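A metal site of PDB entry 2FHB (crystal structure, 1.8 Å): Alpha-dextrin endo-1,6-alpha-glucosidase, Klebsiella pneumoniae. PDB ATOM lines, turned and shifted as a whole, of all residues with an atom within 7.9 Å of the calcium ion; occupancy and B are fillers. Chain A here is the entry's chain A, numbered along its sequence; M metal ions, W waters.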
ATOM      1  N   LEU A 961     -16.731  29.234 -11.591  1.00  0.00           N
ATOM      2  CA  LEU A 961     -16.438  30.193 -12.653  1.00  0.00           C
ATOM      3  C   LEU A 961     -17.642  31.093 -12.972  1.00  0.00           C
ATOM      4  O   LEU A 961     -17.461  32.218 -13.441  1.00  0.00           O
ATOM      5  CB  LEU A 961     -15.959  29.472 -13.910  1.00  0.00           C
ATOM      6  CG  LEU A 961     -14.667  28.672 -13.750  1.00  0.00           C
ATOM      7  CD1 LEU A 961     -14.327  27.950 -15.052  1.00  0.00           C
ATOM      8  CD2 LEU A 961     -13.527  29.600 -13.353  1.00  0.00           C
ATOM      9  N   ARG A 973     -10.825  37.101 -16.182  1.00  0.00           N
ATOM     10  CA  ARG A 973     -11.296  35.835 -16.736  1.00  0.00           C
ATOM     11  C   ARG A 973     -12.456  35.847 -17.737  1.00  0.00           C
ATOM     12  O   ARG A 973     -12.555  34.930 -18.554  1.00  0.00           O
ATOM     13  CB  ARG A 973     -11.669  34.890 -15.594  1.00  0.00           C
ATOM     14  CG  ARG A 973     -10.546  34.574 -14.641  1.00  0.00           C
ATOM     15  CD  ARG A 973     -11.047  33.790 -13.433  1.00  0.00           C
ATOM     16  NE  ARG A 973      -9.961  33.482 -12.503  1.00  0.00           N
ATOM     17  CZ  ARG A 973      -9.373  32.300 -12.386  1.00  0.00           C
ATOM     18  NH1 ARG A 973      -9.751  31.280 -13.143  1.00  0.00           N
ATOM     19  NH2 ARG A 973      -8.390  32.130 -11.513  1.00  0.00           N
ATOM     20  N   ASP A 993     -12.359  32.100 -18.410  1.00  0.00           N
ATOM     21  CA  ASP A 993     -11.030  31.474 -18.352  1.00  0.00           C
ATOM     22  C   ASP A 993     -10.641  30.863 -17.005  1.00  0.00           C
ATOM     23  O   ASP A 993     -10.946  31.403 -15.937  1.00  0.00           O
ATOM     24  CB  ASP A 993      -9.976  32.517 -18.751  1.00  0.00           C
ATOM     25  CG  ASP A 993      -8.609  31.893 -19.014  1.00  0.00           C
ATOM     26  OD1 ASP A 993      -7.627  32.663 -19.098  1.00  0.00           O
ATOM     27  OD2 ASP A 993      -8.510  30.656 -19.135  1.00  0.00           O
ATOM     28  N   ASP A 994      -9.974  29.723 -17.064  1.00  0.00           N
ATOM     29  CA  ASP A 994      -9.486  29.070 -15.862  1.00  0.00           C
ATOM     30  C   ASP A 994      -8.104  28.512 -16.190  1.00  0.00           C
ATOM     31  O   ASP A 994      -7.574  27.654 -15.472  1.00  0.00           O
ATOM     32  CB  ASP A 994     -10.425  27.943 -15.412  1.00  0.00           C
ATOM     33  CG  ASP A 994     -10.192  27.554 -13.959  1.00  0.00           C
ATOM     34  OD1 ASP A 994     -10.083  28.462 -13.110  1.00  0.00           O
ATOM     35  OD2 ASP A 994     -10.109  26.349 -13.660  1.00  0.00           O
ATOM     36  N   GLY A 995      -7.526  29.017 -17.277  1.00  0.00           N
ATOM     37  CA  GLY A 995      -6.210  28.587 -17.708  1.00  0.00           C
ATOM     38  C   GLY A 995      -5.085  29.280 -16.971  1.00  0.00           C
ATOM     39  O   GLY A 995      -5.312  30.058 -16.053  1.00  0.00           O
ATOM     40  N   MET A 996      -3.852  28.991 -17.388  1.00  0.00           N
ATOM     41  CA  MET A 996      -2.661  29.552 -16.771  1.00  0.00           C
ATOM     42  C   MET A 996      -2.568  31.076 -16.756  1.00  0.00           C
ATOM     43  O   MET A 996      -1.999  31.650 -15.822  1.00  0.00           O
ATOM     44  CB  MET A 996      -1.406  28.984 -17.454  1.00  0.00           C
ATOM     45  CG  MET A 996      -1.298  27.468 -17.389  1.00  0.00           C
ATOM     46  SD  MET A 996       0.121  26.821 -18.301  1.00  0.00           S
ATOM     47  CE  MET A 996      -0.543  26.768 -19.976  1.00  0.00           C
ATOM     48  N   GLY A 999      -4.533  32.681 -13.785  1.00  0.00           N
ATOM     49  CA  GLY A 999      -3.957  32.509 -12.464  1.00  0.00           C
ATOM     50  C   GLY A 999      -4.202  31.096 -11.979  1.00  0.00           C
ATOM     51  O   GLY A 999      -3.930  30.132 -12.698  1.00  0.00           O
ATOM     52  N   ALA A1000      -4.714  30.967 -10.761  1.00  0.00           N
ATOM     53  CA  ALA A1000      -4.989  29.661 -10.188  1.00  0.00           C
ATOM     54  C   ALA A1000      -6.188  28.994 -10.844  1.00  0.00           C
ATOM     55  O   ALA A1000      -7.065  29.657 -11.391  1.00  0.00           O
ATOM     56  CB  ALA A1000      -5.239  29.812  -8.692  1.00  0.00           C
ATOM     57  N   SER A1001      -6.210  27.667 -10.792  1.00  0.00           N
ATOM     58  CA  SER A1001      -7.305  26.892 -11.363  1.00  0.00           C
ATOM     59  C   SER A1001      -8.378  26.791 -10.291  1.00  0.00           C
ATOM     60  O   SER A1001      -8.187  26.127  -9.273  1.00  0.00           O
ATOM     61  CB  SER A1001      -6.829  25.496 -11.759  1.00  0.00           C
ATOM     62  OG  SER A1001      -7.913  24.682 -12.149  1.00  0.00           O
ATOM     63  N   LEU A1002      -9.499  27.469 -10.511  1.00  0.00           N
ATOM     64  CA  LEU A1002     -10.600  27.458  -9.547  1.00  0.00           C
ATOM     65  C   LEU A1002     -11.481  26.225  -9.711  1.00  0.00           C
ATOM     66  O   LEU A1002     -12.177  25.837  -8.779  1.00  0.00           O
ATOM     67  CB  LEU A1002     -11.444  28.727  -9.716  1.00  0.00           C
ATOM     68  CG  LEU A1002     -10.713  30.056  -9.519  1.00  0.00           C
ATOM     69  CD1 LEU A1002     -11.675  31.211  -9.731  1.00  0.00           C
ATOM     70  CD2 LEU A1002     -10.115  30.102  -8.117  1.00  0.00           C
ATOM     71  N   ASP A1003     -11.441  25.628 -10.887  1.00  0.00           N
ATOM     72  CA  ASP A1003     -12.235  24.441 -11.176  1.00  0.00           C
ATOM     73  C   ASP A1003     -11.295  23.349 -11.676  1.00  0.00           C
ATOM     74  O   ASP A1003     -10.633  23.513 -12.708  1.00  0.00           O
ATOM     75  CB  ASP A1003     -13.304  24.769 -12.219  1.00  0.00           C
ATOM     76  CG  ASP A1003     -14.333  23.660 -12.391  1.00  0.00           C
ATOM     77  OD1 ASP A1003     -15.484  23.970 -12.770  1.00  0.00           O
ATOM     78  OD2 ASP A1003     -13.996  22.483 -12.151  1.00  0.00           O
ATOM     79  N   SER A1004     -11.230  22.241 -10.950  1.00  0.00           N
ATOM     80  CA  SER A1004     -10.342  21.146 -11.302  1.00  0.00           C
ATOM     81  C   SER A1004     -10.832  20.294 -12.458  1.00  0.00           C
ATOM     82  O   SER A1004     -10.121  19.422 -12.930  1.00  0.00           O
ATOM     83  CB  SER A1004     -10.109  20.245 -10.075  1.00  0.00           C
ATOM     84  OG  SER A1004     -11.322  19.654  -9.647  1.00  0.00           O
ATOM     85  N   ARG A1005     -12.055  20.549 -12.913  1.00  0.00           N
ATOM     86  CA  ARG A1005     -12.606  19.769 -14.014  1.00  0.00           C
ATOM     87  C   ARG A1005     -12.505  20.465 -15.366  1.00  0.00           C
ATOM     88  O   ARG A1005     -12.618  19.812 -16.417  1.00  0.00           O
ATOM     89  CB  ARG A1005     -14.072  19.426 -13.732  1.00  0.00           C
ATOM     90  CG  ARG A1005     -14.287  18.680 -12.424  1.00  0.00           C
ATOM     91  CD  ARG A1005     -15.740  18.261 -12.259  1.00  0.00           C
ATOM     92  NE  ARG A1005     -15.956  17.593 -10.970  1.00  0.00           N
ATOM     93  CZ  ARG A1005     -17.116  17.083 -10.577  1.00  0.00           C
ATOM     94  NH1 ARG A1005     -17.211  16.495  -9.389  1.00  0.00           N
ATOM     95  NH2 ARG A1005     -18.179  17.141 -11.366  1.00  0.00           N
ATOM     96  N   VAL A1006     -12.273  21.773 -15.362  1.00  0.00           N
ATOM     97  CA  VAL A1006     -12.198  22.506 -16.618  1.00  0.00           C
ATOM     98  C   VAL A1006     -11.115  23.586 -16.667  1.00  0.00           C
ATOM     99  O   VAL A1006     -10.709  24.113 -15.640  1.00  0.00           O
ATOM    100  CB  VAL A1006     -13.558  23.203 -16.947  1.00  0.00           C
ATOM    101  CG1 VAL A1006     -14.694  22.204 -16.818  1.00  0.00           C
ATOM    102  CG2 VAL A1006     -13.779  24.381 -15.998  1.00  0.00           C
ATOM    103  N   ASP A1007     -10.676  23.907 -17.876  1.00  0.00           N
ATOM    104  CA  ASP A1007      -9.675  24.949 -18.082  1.00  0.00           C
ATOM    105  C   ASP A1007     -10.408  26.185 -18.580  1.00  0.00           C
ATOM    106  O   ASP A1007      -9.797  27.232 -18.802  1.00  0.00           O
ATOM    107  CB  ASP A1007      -8.637  24.526 -19.126  1.00  0.00           C
ATOM    108  CG  ASP A1007      -7.639  23.516 -18.595  1.00  0.00           C
ATOM    109  OD1 ASP A1007      -7.064  23.776 -17.515  1.00  0.00           O
ATOM    110  OD2 ASP A1007      -7.434  22.477 -19.255  1.00  0.00           O
ATOM    111  N   GLY A1008     -11.714  26.056 -18.772  1.00  0.00           N
ATOM    112  CA  GLY A1008     -12.517  27.173 -19.248  1.00  0.00           C
ATOM    113  C   GLY A1008     -13.950  26.779 -19.560  1.00  0.00           C
ATOM    114  O   GLY A1008     -14.265  25.600 -19.724  1.00  0.00           O
ATOM    115  N   LEU A1068     -13.947  23.134 -21.410  1.00  0.00           N
ATOM    116  CA  LEU A1068     -12.655  22.609 -21.833  1.00  0.00           C
ATOM    117  C   LEU A1068     -12.190  21.683 -20.724  1.00  0.00           C
ATOM    118  O   LEU A1068     -11.815  22.139 -19.640  1.00  0.00           O
ATOM    119  CB  LEU A1068     -11.635  23.735 -22.012  1.00  0.00           C
ATOM    120  CG  LEU A1068     -11.819  24.730 -23.161  1.00  0.00           C
ATOM    121  CD1 LEU A1068     -10.689  25.748 -23.156  1.00  0.00           C
ATOM    122  CD2 LEU A1068     -11.844  23.965 -24.477  1.00  0.00           C
ATOM    123  N   PRO A1069     -12.238  20.360 -20.960  1.00  0.00           N
ATOM    124  CA  PRO A1069     -11.805  19.413 -19.936  1.00  0.00           C
ATOM    125  C   PRO A1069     -10.335  19.634 -19.551  1.00  0.00           C
ATOM    126  O   PRO A1069      -9.480  19.842 -20.420  1.00  0.00           O
ATOM    127  CB  PRO A1069     -12.058  18.061 -20.591  1.00  0.00           C
ATOM    128  CG  PRO A1069     -11.866  18.349 -22.044  1.00  0.00           C
ATOM    129  CD  PRO A1069     -12.584  19.657 -22.207  1.00  0.00           C
ATOM    130  N   GLN A1070     -10.060  19.582 -18.256  1.00  0.00           N
ATOM    131  CA  GLN A1070      -8.705  19.800 -17.761  1.00  0.00           C
ATOM    132  C   GLN A1070      -7.905  18.501 -17.670  1.00  0.00           C
ATOM    133  O   GLN A1070      -8.393  17.499 -17.149  1.00  0.00           O
ATOM    134  CB  GLN A1070      -8.761  20.456 -16.384  1.00  0.00           C
ATOM    135  CG  GLN A1070      -7.422  20.910 -15.834  1.00  0.00           C
ATOM    136  CD  GLN A1070      -7.579  21.790 -14.614  1.00  0.00           C
ATOM    137  OE1 GLN A1070      -8.375  22.725 -14.619  1.00  0.00           O
ATOM    138  NE2 GLN A1070      -6.832  21.497 -13.555  1.00  0.00           N
ATOM    139  N   GLY A1071      -6.689  18.536 -18.194  1.00  0.00           N
ATOM    140  CA  GLY A1071      -5.833  17.362 -18.170  1.00  0.00           C
ATOM    141  C   GLY A1071      -5.054  17.228 -16.881  1.00  0.00           C
ATOM    142  O   GLY A1071      -5.506  17.659 -15.827  1.00  0.00           O
ATOM    143  N   SER A1073      -2.383  18.755 -15.960  1.00  0.00           N
ATOM    144  CA  SER A1073      -2.009  20.069 -15.449  1.00  0.00           C
ATOM    145  C   SER A1073      -2.939  21.139 -15.989  1.00  0.00           C
ATOM    146  O   SER A1073      -3.770  20.875 -16.864  1.00  0.00           O
ATOM    147  CB  SER A1073      -0.566  20.398 -15.836  1.00  0.00           C
ATOM    148  OG  SER A1073      -0.416  20.430 -17.244  1.00  0.00           O
ATOM    149  N   GLN A1074      -2.823  22.358 -15.466  1.00  0.00           N
ATOM    150  CA  GLN A1074      -3.642  23.464 -15.902  1.00  0.00           C
ATOM    151  C   GLN A1074      -3.348  23.735 -17.386  1.00  0.00           C
ATOM    152  O   GLN A1074      -2.183  23.858 -17.771  1.00  0.00           O
ATOM    153  CB  GLN A1074      -3.333  24.709 -15.071  1.00  0.00           C
ATOM    154  CG  GLN A1074      -4.279  25.882 -15.301  1.00  0.00           C
ATOM    155  CD  GLN A1074      -4.026  27.030 -14.351  1.00  0.00           C
ATOM    156  OE1 GLN A1074      -4.783  28.012 -14.322  1.00  0.00           O
ATOM    157  NE2 GLN A1074      -2.966  26.931 -13.555  1.00  0.00           N
ATOM    158  N   GLY A1075      -4.395  23.811 -18.193  1.00  0.00           N
ATOM    159  CA  GLY A1075      -4.216  24.053 -19.619  1.00  0.00           C
ATOM    160  C   GLY A1075      -4.123  25.505 -20.013  1.00  0.00           C
ATOM    161  O   GLY A1075      -3.924  26.382 -19.163  1.00  0.00           O
HETATM  162 CA    CA M   1      -9.190  24.486 -14.021  1.00  0.00          CA
HETATM  163  O   HOH W   1      -7.710  25.176 -15.378  1.00  0.00           O
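The side-chain carboxylate (OD1) of Asp 1007 sits close to the side-chain amide oxygen (OE1) of Gln 1070.
O of Arg 1005 is in hydrogen-bond range of N of Gln 1070.
The backbone carbonyl oxygen (O) of Asp 1007 sits at hydrogen-bond distance from the backbone NH (N) of Asp 994.
The side-chain carboxylate (OD1) of Asp 994 is in hydrogen-bond range of the backbone NH (N) of Leu 1002, at 2.8 Å.
The backbone carbonyl oxygen (O) of Asp 994 sits close to the side-chain amide oxygen (OE1) of Gln 1074.
The side-chain carboxylate (OD1) of Asp 994 is in salt-bridge range of the guanidinium group (NH1) of Arg 973 (2.8 Å).
OD2 of Asp 1003 is in hydrogen-bond range of N of Arg 1005.
OE1 of Gln 1070 binds the calcium ion, 2.0 Å away.
The side-chain carboxylate (OD2) of Asp 994 is bound to the calcium ion (2.1 Å).
Water W1 binds the calcium ion (2.1 Å).
The calcium ion is bound by O of Asp 1003, at 2.2 Å.
The calcium ion is bound by the backbone carbonyl oxygen (O) of Val 1006 (2.3 Å).
The calcium ion is bound by OG of Ser 1001, at 2.3 Å.
Water W1 bridges O of Asp 994 (2.5 Å) and OD1 of Asp 1007 (2.6 Å).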
